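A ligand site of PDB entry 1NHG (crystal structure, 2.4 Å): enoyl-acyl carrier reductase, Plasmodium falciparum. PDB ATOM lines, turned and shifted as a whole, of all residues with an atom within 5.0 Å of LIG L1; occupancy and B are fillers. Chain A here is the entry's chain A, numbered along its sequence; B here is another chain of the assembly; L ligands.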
ATOM      1  N   GLY A   8      27.596  -3.017 -11.451  1.00  0.00           N
ATOM      2  CA  GLY A   8      26.454  -3.532 -12.191  1.00  0.00           C
ATOM      3  C   GLY A   8      25.094  -3.297 -11.561  1.00  0.00           C
ATOM      4  O   GLY A   8      24.254  -4.189 -11.549  1.00  0.00           O
ATOM      5  N   ILE A   9      24.878  -2.104 -11.028  1.00  0.00           N
ATOM      6  CA  ILE A   9      23.591  -1.769 -10.440  1.00  0.00           C
ATOM      7  C   ILE A   9      22.970  -0.667 -11.295  1.00  0.00           C
ATOM      8  O   ILE A   9      23.634   0.320 -11.626  1.00  0.00           O
ATOM      9  CB  ILE A   9      23.732  -1.275  -8.990  1.00  0.00           C
ATOM     10  CG1 ILE A   9      24.182  -2.441  -8.102  1.00  0.00           C
ATOM     11  CG2 ILE A   9      22.408  -0.731  -8.479  1.00  0.00           C
ATOM     12  CD1 ILE A   9      24.176  -2.142  -6.630  1.00  0.00           C
ATOM     13  N   GLY A  10      21.709  -0.854 -11.650  1.00  0.00           N
ATOM     14  CA  GLY A  10      21.017   0.131 -12.462  1.00  0.00           C
ATOM     15  C   GLY A  10      19.642   0.415 -11.897  1.00  0.00           C
ATOM     16  O   GLY A  10      18.943   1.316 -12.339  1.00  0.00           O
ATOM     17  N   ASP A  11      19.262  -0.355 -10.892  1.00  0.00           N
ATOM     18  CA  ASP A  11      17.968  -0.194 -10.258  1.00  0.00           C
ATOM     19  C   ASP A  11      17.878  -1.173  -9.099  1.00  0.00           C
ATOM     20  O   ASP A  11      18.897  -1.756  -8.697  1.00  0.00           O
ATOM     21  CB  ASP A  11      16.843  -0.470 -11.265  1.00  0.00           C
ATOM     22  CG  ASP A  11      16.978  -1.825 -11.917  1.00  0.00           C
ATOM     23  OD1 ASP A  11      17.005  -2.843 -11.185  1.00  0.00           O
ATOM     24  OD2 ASP A  11      17.063  -1.883 -13.158  1.00  0.00           O
ATOM     25  N   ASN A  13      15.774  -3.882  -9.107  1.00  0.00           N
ATOM     26  CA  ASN A  13      15.130  -5.113  -9.535  1.00  0.00           C
ATOM     27  C   ASN A  13      16.097  -6.204  -9.965  1.00  0.00           C
ATOM     28  O   ASN A  13      15.674  -7.294 -10.362  1.00  0.00           O
ATOM     29  CB  ASN A  13      14.156  -4.818 -10.685  1.00  0.00           C
ATOM     30  CG  ASN A  13      13.163  -3.742 -10.319  1.00  0.00           C
ATOM     31  OD1 ASN A  13      12.542  -3.787  -9.245  1.00  0.00           O
ATOM     32  ND2 ASN A  13      12.995  -2.760 -11.195  1.00  0.00           N
ATOM     33  N   GLY A  14      17.390  -5.917  -9.874  1.00  0.00           N
ATOM     34  CA  GLY A  14      18.374  -6.907 -10.271  1.00  0.00           C
ATOM     35  C   GLY A  14      19.013  -7.609  -9.091  1.00  0.00           C
ATOM     36  O   GLY A  14      18.657  -7.379  -7.932  1.00  0.00           O
ATOM     37  N   TYR A  15      19.959  -8.496  -9.393  1.00  0.00           N
ATOM     38  CA  TYR A  15      20.665  -9.241  -8.366  1.00  0.00           C
ATOM     39  C   TYR A  15      21.632  -8.333  -7.597  1.00  0.00           C
ATOM     40  O   TYR A  15      21.889  -8.542  -6.411  1.00  0.00           O
ATOM     41  CB  TYR A  15      21.431 -10.406  -8.985  1.00  0.00           C
ATOM     42  CG  TYR A  15      20.576 -11.643  -9.205  1.00  0.00           C
ATOM     43  CD1 TYR A  15      19.914 -12.245  -8.141  1.00  0.00           C
ATOM     44  CD2 TYR A  15      20.473 -12.226 -10.469  1.00  0.00           C
ATOM     45  CE1 TYR A  15      19.160 -13.399  -8.312  1.00  0.00           C
ATOM     46  CE2 TYR A  15      19.718 -13.394 -10.660  1.00  0.00           C
ATOM     47  CZ  TYR A  15      19.068 -13.965  -9.582  1.00  0.00           C
ATOM     48  OH  TYR A  15      18.334 -15.112  -9.745  1.00  0.00           O
ATOM     49  N   GLY A  16      22.173  -7.339  -8.285  1.00  0.00           N
ATOM     50  CA  GLY A  16      23.088  -6.416  -7.638  1.00  0.00           C
ATOM     51  C   GLY A  16      22.488  -5.868  -6.364  1.00  0.00           C
ATOM     52  O   GLY A  16      23.133  -5.835  -5.315  1.00  0.00           O
ATOM     53  N   TRP A  35      26.531   2.062 -14.560  1.00  0.00           N
ATOM     54  CA  TRP A  35      26.804   2.247 -15.979  1.00  0.00           C
ATOM     55  C   TRP A  35      26.394   3.680 -16.362  1.00  0.00           C
ATOM     56  O   TRP A  35      25.233   4.057 -16.246  1.00  0.00           O
ATOM     57  CB  TRP A  35      26.008   1.205 -16.769  1.00  0.00           C
ATOM     58  CG  TRP A  35      26.355   1.124 -18.215  1.00  0.00           C
ATOM     59  CD1 TRP A  35      27.597   1.233 -18.765  1.00  0.00           C
ATOM     60  CD2 TRP A  35      25.449   0.859 -19.295  1.00  0.00           C
ATOM     61  NE1 TRP A  35      27.527   1.051 -20.121  1.00  0.00           N
ATOM     62  CE2 TRP A  35      26.230   0.815 -20.476  1.00  0.00           C
ATOM     63  CE3 TRP A  35      24.073   0.650 -19.376  1.00  0.00           C
ATOM     64  CZ2 TRP A  35      25.667   0.570 -21.737  1.00  0.00           C
ATOM     65  CZ3 TRP A  35      23.510   0.406 -20.638  1.00  0.00           C
ATOM     66  CH2 TRP A  35      24.302   0.363 -21.797  1.00  0.00           C
ATOM     67  N   VAL A  38      22.831   5.154 -17.474  1.00  0.00           N
ATOM     68  CA  VAL A  38      21.713   5.219 -16.550  1.00  0.00           C
ATOM     69  C   VAL A  38      22.074   5.828 -15.196  1.00  0.00           C
ATOM     70  O   VAL A  38      21.275   5.789 -14.254  1.00  0.00           O
ATOM     71  CB  VAL A  38      21.088   3.810 -16.308  1.00  0.00           C
ATOM     72  CG1 VAL A  38      20.811   3.136 -17.637  1.00  0.00           C
ATOM     73  CG2 VAL A  38      22.006   2.961 -15.458  1.00  0.00           C
ATOM     74  N   PHE A  71      30.502   4.010 -13.784  1.00  0.00           N
ATOM     75  CA  PHE A  71      31.462   2.956 -14.088  1.00  0.00           C
ATOM     76  C   PHE A  71      31.099   2.199 -15.354  1.00  0.00           C
ATOM     77  O   PHE A  71      29.972   1.708 -15.472  1.00  0.00           O
ATOM     78  CB  PHE A  71      31.511   1.987 -12.911  1.00  0.00           C
ATOM     79  CG  PHE A  71      32.312   0.749 -13.152  1.00  0.00           C
ATOM     80  CD1 PHE A  71      33.693   0.740 -12.952  1.00  0.00           C
ATOM     81  CD2 PHE A  71      31.698  -0.426 -13.559  1.00  0.00           C
ATOM     82  CE1 PHE A  71      34.440  -0.421 -13.132  1.00  0.00           C
ATOM     83  CE2 PHE A  71      32.426  -1.595 -13.746  1.00  0.00           C
ATOM     84  CZ  PHE A  71      33.796  -1.593 -13.533  1.00  0.00           C
ATOM     85  N   ASP A  72      32.036   2.096 -16.289  1.00  0.00           N
ATOM     86  CA  ASP A  72      31.792   1.370 -17.524  1.00  0.00           C
ATOM     87  C   ASP A  72      32.820   0.252 -17.655  1.00  0.00           C
ATOM     88  O   ASP A  72      34.023   0.507 -17.764  1.00  0.00           O
ATOM     89  CB  ASP A  72      31.877   2.295 -18.746  1.00  0.00           C
ATOM     90  CG  ASP A  72      31.298   1.660 -19.985  1.00  0.00           C
ATOM     91  OD1 ASP A  72      31.629   0.486 -20.261  1.00  0.00           O
ATOM     92  OD2 ASP A  72      30.511   2.330 -20.686  1.00  0.00           O
ATOM     93  N   ALA A  73      32.339  -0.985 -17.654  1.00  0.00           N
ATOM     94  CA  ALA A  73      33.199  -2.154 -17.732  1.00  0.00           C
ATOM     95  C   ALA A  73      33.869  -2.389 -19.074  1.00  0.00           C
ATOM     96  O   ALA A  73      34.716  -3.271 -19.216  1.00  0.00           O
ATOM     97  CB  ALA A  73      32.412  -3.397 -17.328  1.00  0.00           C
ATOM     98  N   SER A  74      33.507  -1.594 -20.071  1.00  0.00           N
ATOM     99  CA  SER A  74      34.091  -1.763 -21.396  1.00  0.00           C
ATOM    100  C   SER A  74      35.362  -0.934 -21.622  1.00  0.00           C
ATOM    101  O   SER A  74      35.957  -0.996 -22.701  1.00  0.00           O
ATOM    102  CB  SER A  74      33.055  -1.444 -22.478  1.00  0.00           C
ATOM    103  OG  SER A  74      32.640  -0.098 -22.386  1.00  0.00           O
ATOM    104  N   SER A 119      28.560  -7.932 -11.214  1.00  0.00           N
ATOM    105  CA  SER A 119      27.169  -8.274 -11.449  1.00  0.00           C
ATOM    106  C   SER A 119      26.641  -7.591 -12.709  1.00  0.00           C
ATOM    107  O   SER A 119      25.570  -6.998 -12.702  1.00  0.00           O
ATOM    108  CB  SER A 119      26.329  -7.846 -10.236  1.00  0.00           C
ATOM    109  OG  SER A 119      24.972  -8.212 -10.384  1.00  0.00           O
ATOM    110  N   LEU A 120      27.408  -7.681 -13.791  1.00  0.00           N
ATOM    111  CA  LEU A 120      27.008  -7.053 -15.033  1.00  0.00           C
ATOM    112  C   LEU A 120      27.218  -7.962 -16.238  1.00  0.00           C
ATOM    113  O   LEU A 120      27.962  -8.926 -16.182  1.00  0.00           O
ATOM    114  CB  LEU A 120      27.800  -5.759 -15.225  1.00  0.00           C
ATOM    115  CG  LEU A 120      29.304  -5.949 -15.407  1.00  0.00           C
ATOM    116  CD1 LEU A 120      29.654  -5.746 -16.874  1.00  0.00           C
ATOM    117  CD2 LEU A 120      30.053  -4.946 -14.547  1.00  0.00           C
ATOM    118  N   ALA A 121      26.535  -7.634 -17.324  1.00  0.00           N
ATOM    119  CA  ALA A 121      26.635  -8.387 -18.571  1.00  0.00           C
ATOM    120  C   ALA A 121      25.992  -7.561 -19.675  1.00  0.00           C
ATOM    121  O   ALA A 121      25.161  -6.698 -19.406  1.00  0.00           O
ATOM    122  CB  ALA A 121      25.932  -9.738 -18.446  1.00  0.00           C
ATOM    123  N   ASN A 122      26.382  -7.812 -20.912  1.00  0.00           N
ATOM    124  CA  ASN A 122      25.815  -7.072 -22.026  1.00  0.00           C
ATOM    125  C   ASN A 122      26.172  -7.769 -23.310  1.00  0.00           C
ATOM    126  O   ASN A 122      27.184  -8.475 -23.387  1.00  0.00           O
ATOM    127  CB  ASN A 122      26.337  -5.639 -22.038  1.00  0.00           C
ATOM    128  CG  ASN A 122      25.308  -4.636 -22.534  1.00  0.00           C
ATOM    129  OD1 ASN A 122      25.355  -3.454 -22.170  1.00  0.00           O
ATOM    130  ND2 ASN A 122      24.376  -5.100 -23.355  1.00  0.00           N
ATOM    131  N   LYS A 144      32.340  -7.203 -22.720  1.00  0.00           N
ATOM    132  CA  LYS A 144      31.555  -6.638 -21.636  1.00  0.00           C
ATOM    133  C   LYS A 144      31.240  -7.619 -20.504  1.00  0.00           C
ATOM    134  O   LYS A 144      31.359  -7.280 -19.327  1.00  0.00           O
ATOM    135  CB  LYS A 144      30.230  -6.087 -22.172  1.00  0.00           C
ATOM    136  CG  LYS A 144      30.281  -4.660 -22.705  1.00  0.00           C
ATOM    137  CD  LYS A 144      31.043  -4.547 -23.996  1.00  0.00           C
ATOM    138  CE  LYS A 144      30.884  -3.139 -24.592  1.00  0.00           C
ATOM    139  NZ  LYS A 144      29.473  -2.853 -24.961  1.00  0.00           N
ATOM    140  N   LEU A 169      28.256 -13.387 -11.303  1.00  0.00           N
ATOM    141  CA  LEU A 169      27.069 -14.201 -11.543  1.00  0.00           C
ATOM    142  C   LEU A 169      27.132 -14.806 -12.949  1.00  0.00           C
ATOM    143  O   LEU A 169      27.569 -14.161 -13.901  1.00  0.00           O
ATOM    144  CB  LEU A 169      25.791 -13.360 -11.426  1.00  0.00           C
ATOM    145  CG  LEU A 169      25.388 -12.702 -10.100  1.00  0.00           C
ATOM    146  CD1 LEU A 169      25.402 -13.723  -8.980  1.00  0.00           C
ATOM    147  CD2 LEU A 169      26.324 -11.558  -9.776  1.00  0.00           C
ATOM    148  N   THR A 170      26.699 -16.052 -13.067  1.00  0.00           N
ATOM    149  CA  THR A 170      26.697 -16.736 -14.339  1.00  0.00           C
ATOM    150  C   THR A 170      25.352 -17.431 -14.508  1.00  0.00           C
ATOM    151  O   THR A 170      24.482 -17.329 -13.642  1.00  0.00           O
ATOM    152  CB  THR A 170      27.855 -17.774 -14.412  1.00  0.00           C
ATOM    153  OG1 THR A 170      27.922 -18.323 -15.728  1.00  0.00           O
ATOM    154  CG2 THR A 170      27.653 -18.897 -13.394  1.00  0.00           C
ATOM    155  N   TYR A 171      25.180 -18.135 -15.621  1.00  0.00           N
ATOM    156  CA  TYR A 171      23.920 -18.807 -15.894  1.00  0.00           C
ATOM    157  C   TYR A 171      24.195 -20.170 -16.528  1.00  0.00           C
ATOM    158  O   TYR A 171      25.125 -20.311 -17.321  1.00  0.00           O
ATOM    159  CB  TYR A 171      23.062 -17.919 -16.822  1.00  0.00           C
ATOM    160  CG  TYR A 171      21.698 -18.487 -17.163  1.00  0.00           C
ATOM    161  CD1 TYR A 171      20.816 -18.871 -16.152  1.00  0.00           C
ATOM    162  CD2 TYR A 171      21.300 -18.646 -18.493  1.00  0.00           C
ATOM    163  CE1 TYR A 171      19.567 -19.403 -16.456  1.00  0.00           C
ATOM    164  CE2 TYR A 171      20.050 -19.178 -18.798  1.00  0.00           C
ATOM    165  CZ  TYR A 171      19.193 -19.559 -17.786  1.00  0.00           C
ATOM    166  OH  TYR A 171      17.974 -20.111 -18.082  1.00  0.00           O
ATOM    167  N   TYR A 181      18.908 -17.700 -25.428  1.00  0.00           N
ATOM    168  CA  TYR A 181      20.037 -17.050 -24.762  1.00  0.00           C
ATOM    169  C   TYR A 181      21.137 -16.928 -25.803  1.00  0.00           C
ATOM    170  O   TYR A 181      22.139 -17.625 -25.718  1.00  0.00           O
ATOM    171  CB  TYR A 181      20.504 -17.905 -23.598  1.00  0.00           C
ATOM    172  CG  TYR A 181      21.325 -17.179 -22.566  1.00  0.00           C
ATOM    173  CD1 TYR A 181      20.756 -16.209 -21.740  1.00  0.00           C
ATOM    174  CD2 TYR A 181      22.681 -17.492 -22.374  1.00  0.00           C
ATOM    175  CE1 TYR A 181      21.501 -15.580 -20.744  1.00  0.00           C
ATOM    176  CE2 TYR A 181      23.427 -16.864 -21.393  1.00  0.00           C
ATOM    177  CZ  TYR A 181      22.831 -15.908 -20.574  1.00  0.00           C
ATOM    178  OH  TYR A 181      23.569 -15.332 -19.570  1.00  0.00           O
ATOM    179  N   MET A 185      26.050 -14.819 -25.424  1.00  0.00           N
ATOM    180  CA  MET A 185      26.000 -14.758 -23.969  1.00  0.00           C
ATOM    181  C   MET A 185      26.362 -16.109 -23.348  1.00  0.00           C
ATOM    182  O   MET A 185      27.008 -16.168 -22.297  1.00  0.00           O
ATOM    183  CB  MET A 185      24.604 -14.299 -23.500  1.00  0.00           C
ATOM    184  CG  MET A 185      24.448 -12.793 -23.496  1.00  0.00           C
ATOM    185  SD  MET A 185      25.784 -11.986 -22.573  1.00  0.00           S
ATOM    186  CE  MET A 185      25.524 -12.716 -20.957  1.00  0.00           C
ATOM    187  N   LYS A 189      29.407 -16.630 -20.729  1.00  0.00           N
ATOM    188  CA  LYS A 189      29.257 -17.269 -19.431  1.00  0.00           C
ATOM    189  C   LYS A 189      30.175 -18.491 -19.308  1.00  0.00           C
ATOM    190  O   LYS A 189      30.717 -18.765 -18.233  1.00  0.00           O
ATOM    191  CB  LYS A 189      27.794 -17.654 -19.199  1.00  0.00           C
ATOM    192  CG  LYS A 189      26.823 -16.465 -19.054  1.00  0.00           C
ATOM    193  CD  LYS A 189      27.181 -15.611 -17.840  1.00  0.00           C
ATOM    194  CE  LYS A 189      26.286 -14.387 -17.743  1.00  0.00           C
ATOM    195  NZ  LYS A 189      26.650 -13.493 -16.601  1.00  0.00           N
ATOM    196  N   ALA A 216      22.996 -18.265 -11.021  1.00  0.00           N
ATOM    197  CA  ALA A 216      21.642 -18.004 -10.539  1.00  0.00           C
ATOM    198  C   ALA A 216      20.520 -18.525 -11.406  1.00  0.00           C
ATOM    199  O   ALA A 216      20.705 -18.832 -12.583  1.00  0.00           O
ATOM    200  CB  ALA A 216      21.475 -16.518 -10.337  1.00  0.00           C
ATOM    201  N   GLY A 217      19.342 -18.631 -10.784  1.00  0.00           N
ATOM    202  CA  GLY A 217      18.144 -19.068 -11.464  1.00  0.00           C
ATOM    203  C   GLY A 217      17.507 -17.828 -12.075  1.00  0.00           C
ATOM    204  O   GLY A 217      18.085 -16.747 -11.971  1.00  0.00           O
ATOM    205  N   PRO A 218      16.309 -17.933 -12.685  1.00  0.00           N
ATOM    206  CA  PRO A 218      15.637 -16.790 -13.316  1.00  0.00           C
ATOM    207  C   PRO A 218      15.094 -15.715 -12.365  1.00  0.00           C
ATOM    208  O   PRO A 218      14.508 -16.025 -11.333  1.00  0.00           O
ATOM    209  CB  PRO A 218      14.494 -17.440 -14.110  1.00  0.00           C
ATOM    210  CG  PRO A 218      14.737 -18.939 -14.013  1.00  0.00           C
ATOM    211  CD  PRO A 218      15.444 -19.114 -12.710  1.00  0.00           C
ATOM    212  N   LEU A 219      15.303 -14.453 -12.742  1.00  0.00           N
ATOM    213  CA  LEU A 219      14.828 -13.317 -11.967  1.00  0.00           C
ATOM    214  C   LEU A 219      14.392 -12.257 -12.979  1.00  0.00           C
ATOM    215  O   LEU A 219      15.182 -11.846 -13.844  1.00  0.00           O
ATOM    216  CB  LEU A 219      15.943 -12.744 -11.073  1.00  0.00           C
ATOM    217  CG  LEU A 219      15.622 -11.480 -10.261  1.00  0.00           C
ATOM    218  CD1 LEU A 219      14.679 -11.825  -9.118  1.00  0.00           C
ATOM    219  CD2 LEU A 219      16.908 -10.885  -9.717  1.00  0.00           C
ATOM    220  N   SER A 221      14.481  -9.284 -14.077  1.00  0.00           N
ATOM    221  CA  SER A 221      15.221  -8.039 -13.930  1.00  0.00           C
ATOM    222  C   SER A 221      15.098  -7.255 -15.232  1.00  0.00           C
ATOM    223  O   SER A 221      14.555  -7.751 -16.219  1.00  0.00           O
ATOM    224  CB  SER A 221      16.697  -8.337 -13.665  1.00  0.00           C
ATOM    225  OG  SER A 221      17.271  -9.023 -14.759  1.00  0.00           O
ATOM    226  N   ARG A 222      15.618  -6.031 -15.239  1.00  0.00           N
ATOM    227  CA  ARG A 222      15.532  -5.200 -16.435  1.00  0.00           C
ATOM    228  C   ARG A 222      16.181  -5.881 -17.640  1.00  0.00           C
ATOM    229  O   ARG A 222      15.576  -5.973 -18.701  1.00  0.00           O
ATOM    230  CB  ARG A 222      16.205  -3.849 -16.200  1.00  0.00           C
ATOM    231  CG  ARG A 222      15.794  -2.833 -17.232  1.00  0.00           C
ATOM    232  CD  ARG A 222      16.639  -1.569 -17.231  1.00  0.00           C
ATOM    233  NE  ARG A 222      16.091  -0.595 -18.166  1.00  0.00           N
ATOM    234  CZ  ARG A 222      15.857  -0.833 -19.462  1.00  0.00           C
ATOM    235  NH1 ARG A 222      16.122  -2.020 -19.980  1.00  0.00           N
ATOM    236  NH2 ARG A 222      15.340   0.119 -20.226  1.00  0.00           N
ATOM    237  N   ALA A 223      17.414  -6.341 -17.462  1.00  0.00           N
ATOM    238  CA  ALA A 223      18.129  -7.006 -18.546  1.00  0.00           C
ATOM    239  C   ALA A 223      17.402  -8.264 -19.011  1.00  0.00           C
ATOM    240  O   ALA A 223      17.369  -8.566 -20.201  1.00  0.00           O
ATOM    241  CB  ALA A 223      19.528  -7.355 -18.105  1.00  0.00           C
ATOM    242  N   ALA A 224      16.837  -9.021 -18.060  1.00  0.00           N
ATOM    243  CA  ALA A 224      16.119 -10.246 -18.384  1.00  0.00           C
ATOM    244  C   ALA A 224      14.948  -9.955 -19.306  1.00  0.00           C
ATOM    245  O   ALA A 224      14.646 -10.725 -20.210  1.00  0.00           O
ATOM    246  CB  ALA A 224      15.633 -10.928 -17.101  1.00  0.00           C
ATOM    247  N   ILE B   4      12.103 -14.627 -20.295  1.00  0.00           N
ATOM    248  CA  ILE B   4      12.176 -14.675 -18.841  1.00  0.00           C
ATOM    249  C   ILE B   4      10.919 -15.206 -18.155  1.00  0.00           C
ATOM    250  O   ILE B   4      11.034 -15.887 -17.132  1.00  0.00           O
ATOM    251  CB  ILE B   4      12.553 -13.294 -18.240  1.00  0.00           C
ATOM    252  CG1 ILE B   4      12.981 -13.472 -16.781  1.00  0.00           C
ATOM    253  CG2 ILE B   4      11.390 -12.325 -18.335  1.00  0.00           C
ATOM    254  CD1 ILE B   4      14.192 -14.376 -16.587  1.00  0.00           C
HETATM  255  P1  LIG L   1      20.497  -6.109 -14.173  1.00  0.00           P
HETATM  256  O1  LIG L   1      19.894  -5.481 -12.965  1.00  0.00           O
HETATM  257  O2  LIG L   1      19.976  -5.660 -15.535  1.00  0.00           O
HETATM  258  O3  LIG L   1      22.093  -5.817 -14.046  1.00  0.00           O
HETATM  259  C1  LIG L   1      23.081  -5.749 -15.110  1.00  0.00           C
HETATM  260  C2  LIG L   1      23.761  -4.420 -15.087  1.00  0.00           C
HETATM  261  O4  LIG L   1      24.943  -4.332 -15.942  1.00  0.00           O
HETATM  262  C3  LIG L   1      22.826  -3.283 -15.520  1.00  0.00           C
HETATM  263  O5  LIG L   1      22.400  -2.613 -14.323  1.00  0.00           O
HETATM  264  C4  LIG L   1      23.669  -2.403 -16.459  1.00  0.00           C
HETATM  265  O6  LIG L   1      23.493  -1.043 -16.134  1.00  0.00           O
HETATM  266  C5  LIG L   1      25.118  -2.957 -16.301  1.00  0.00           C
HETATM  267  N1  LIG L   1      25.900  -2.881 -17.563  1.00  0.00           N
HETATM  268  C6  LIG L   1      25.848  -3.160 -18.916  1.00  0.00           C
HETATM  269  N2  LIG L   1      26.933  -2.857 -19.616  1.00  0.00           N
HETATM  270  C7  LIG L   1      27.781  -2.329 -18.658  1.00  0.00           C
HETATM  271  C8  LIG L   1      29.082  -1.806 -18.734  1.00  0.00           C
HETATM  272  N3  LIG L   1      29.759  -1.704 -19.871  1.00  0.00           N
HETATM  273  N4  LIG L   1      29.660  -1.366 -17.604  1.00  0.00           N
HETATM  274  C9  LIG L   1      29.004  -1.494 -16.429  1.00  0.00           C
HETATM  275  N5  LIG L   1      27.748  -1.886 -16.220  1.00  0.00           N
HETATM  276  C10 LIG L   1      27.173  -2.344 -17.393  1.00  0.00           C
HETATM  277  O7  LIG L   1      20.358  -7.611 -14.405  1.00  0.00           O
HETATM  278  P2  LIG L   1      20.651  -8.825 -13.577  1.00  0.00           P
HETATM  279  O8  LIG L   1      20.476  -8.638 -12.107  1.00  0.00           O
HETATM  280  O9  LIG L   1      19.910  -9.915 -14.244  1.00  0.00           O
HETATM  281  O10 LIG L   1      22.135  -9.188 -14.060  1.00  0.00           O
HETATM  282  C11 LIG L   1      23.302  -9.139 -13.237  1.00  0.00           C
HETATM  283  C12 LIG L   1      24.086 -10.449 -13.462  1.00  0.00           C
HETATM  284  O11 LIG L   1      23.252 -11.592 -13.083  1.00  0.00           O
HETATM  285  C13 LIG L   1      24.461 -10.620 -14.934  1.00  0.00           C
HETATM  286  O12 LIG L   1      25.807 -10.981 -14.961  1.00  0.00           O
HETATM  287  C14 LIG L   1      23.556 -11.723 -15.372  1.00  0.00           C
HETATM  288  O13 LIG L   1      24.128 -12.437 -16.430  1.00  0.00           O
HETATM  289  C15 LIG L   1      23.452 -12.550 -14.125  1.00  0.00           C
HETATM  290  N6  LIG L   1      22.385 -13.548 -14.102  1.00  0.00           N
HETATM  291  C16 LIG L   1      21.035 -13.107 -14.099  1.00  0.00           C
HETATM  292  C17 LIG L   1      19.884 -13.889 -14.118  1.00  0.00           C
HETATM  293  C18 LIG L   1      18.480 -13.447 -14.095  1.00  0.00           C
HETATM  294  O14 LIG L   1      17.455 -14.295 -14.294  1.00  0.00           O
HETATM  295  N7  LIG L   1      18.069 -12.198 -13.936  1.00  0.00           N
HETATM  296  C19 LIG L   1      20.253 -15.228 -14.014  1.00  0.00           C
HETATM  297  C20 LIG L   1      21.565 -15.793 -13.931  1.00  0.00           C
HETATM  298  C21 LIG L   1      22.676 -14.890 -13.993  1.00  0.00           C
HETATM  299  C1  LG2 L   2      20.255 -15.174 -17.560  1.00  0.00           C
HETATM  300  C2  LG2 L   2      18.820 -15.061 -17.502  1.00  0.00           C
HETATM  301  C3  LG2 L   2      21.047 -13.941 -17.659  1.00  0.00           C
HETATM  302  C4  LG2 L   2      20.385 -12.602 -17.708  1.00  0.00           C
HETATM  303  C5  LG2 L   2      18.951 -12.535 -17.655  1.00  0.00           C
HETATM  304  C6  LG2 L   2      18.161 -13.756 -17.549  1.00  0.00           C
HETATM  305  C7  LG2 L   2      22.237  -9.414 -21.502  1.00  0.00           C
HETATM  306  C8  LG2 L   2      22.582  -8.757 -20.199  1.00  0.00           C
HETATM  307  C9  LG2 L   2      22.199  -9.435 -18.977  1.00  0.00           C
HETATM  308  C10 LG2 L   2      21.449 -10.791 -19.072  1.00  0.00           C
HETATM  309  C11 LG2 L   2      21.555 -10.651 -21.527  1.00  0.00           C
HETATM  310  C12 LG2 L   2      21.167 -11.338 -20.418  1.00  0.00           C
HETATM  311  O1  LG2 L   2      21.097 -11.383 -17.808  1.00  0.00           O
HETATM  312 CL1  LG2 L   2      17.873 -16.391 -17.377  1.00  0.00          CL
HETATM  313 CL2  LG2 L   2      22.695  -8.593 -22.888  1.00  0.00          CL
HETATM  314 CL3  LG2 L   2      22.563  -8.725 -17.512  1.00  0.00          CL
HETATM  315  O2  LG2 L   2      22.423 -14.078 -17.712  1.00  0.00           O
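NZ of Lys 189 is in hydrogen-bond range of O of Leu 169 (2.9 Å).
O of Gly 217 sits at hydrogen-bond distance from OH of Tyr 15 (2.8 Å).
OG of Ser 221 is in hydrogen-bond range of N of Ala 224.
The side-chain carboxylate (OD2) of Asp 72 lies within hydrogen-bond range of the indole nitrogen (NE1) of Trp 35 (3.3 Å).
The side-chain carboxylate (OD1) of Asp 72 sits at hydrogen-bond distance from the side-chain hydroxyl (OG) of Ser 74.
The backbone carbonyl oxygen (O) of Thr 170 is in hydrogen-bond range of the backbone NH (N) of Ala 216.
N of Gly 14 is in hydrogen-bond range of OD1 of Asp 11 (3.4 Å).
An oxygen (O13) of LIG L1 is in hydrogen-bond range of an oxygen (O2) of LG2 L2 (2.7 Å).
O of Gly 217 lies close to O14 of LIG L1 (3.4 Å).
Residues that only touch LIG L1: Thr 170 (3.1 Å), Ser 119 (3.2 Å), Pro 218 (3.2 Å), Gly 14 (3.3 Å), Trp 35 (3.4 Å), Ala 216 (3.4 Å), Phe 71 (3.5 Å), Leu 169 (3.5 Å), Gly 8 (3.6 Å), Ala 121 (3.6 Å), Ile 9 (3.6 Å), Ser 74 (3.8 Å), Tyr 171 (3.9 Å) and Ile 4 of chain B (3.99 Å).
Hydrophobic or aromatic side chains that line LIG L1: Tyr 15, Trp 35, Ala 73, Leu 120, Ala 121, Leu 169, Tyr 171, Ala 216, Leu 219, Ala 223 and Ile 4 of chain B.
25 residues have an atom within 4 Å of LIG L1: Gly 8, Ile 9, Gly 10, Gly 14, Tyr 15, Trp 35, Phe 71, Asp 72, Ala 73, Ser 74, Ser 119, Leu 120, Ala 121, Asn 122, Leu 169, Thr 170, Tyr 171, Lys 189, Ala 216, Gly 217, Pro 218, Leu 219, Ser 221, Ala 223 and Ile 4 of chain B.
The backbone NH (N) of Leu 219 is in hydrogen-bond range of an oxygen (O14) of LIG L1 (2.7 Å).
The backbone carbonyl oxygen (O) of Leu 219 is in hydrogen-bond range of a nitrogen (N7) of LIG L1.
N4 of LIG L1 sits at hydrogen-bond distance from N of Ala 73, at 2.7 Å.
NZ of Lys 189 is in hydrogen-bond range of O13 of LIG L1 (2.7 Å).
An oxygen (O8) of LIG L1 lies within hydrogen-bond range of the backbone NH (N) of Tyr 15.
OG of Ser 221 lies within hydrogen-bond range of O9 of LIG L1 (2.8 Å).
OD1 of Asp 72 is in hydrogen-bond range of N3 of LIG L1 (2.9 Å).
A nitrogen (N2) of LIG L1 sits close to the side-chain amide oxygen (OD1) of Asn 122, 3.1 Å away.
An oxygen (O2) of LIG L1 sits close to the backbone NH (N) of Ala 223 (3.3 Å).
O12 of LIG L1 sits at hydrogen-bond distance from O of Leu 120.
The backbone NH (N) of Gly 10 is in hydrogen-bond range of an oxygen (O5) of LIG L1 (3.3 Å).
OH of Tyr 181 lies within hydrogen-bond range of O2 of LG2 L2 (2.5 Å).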
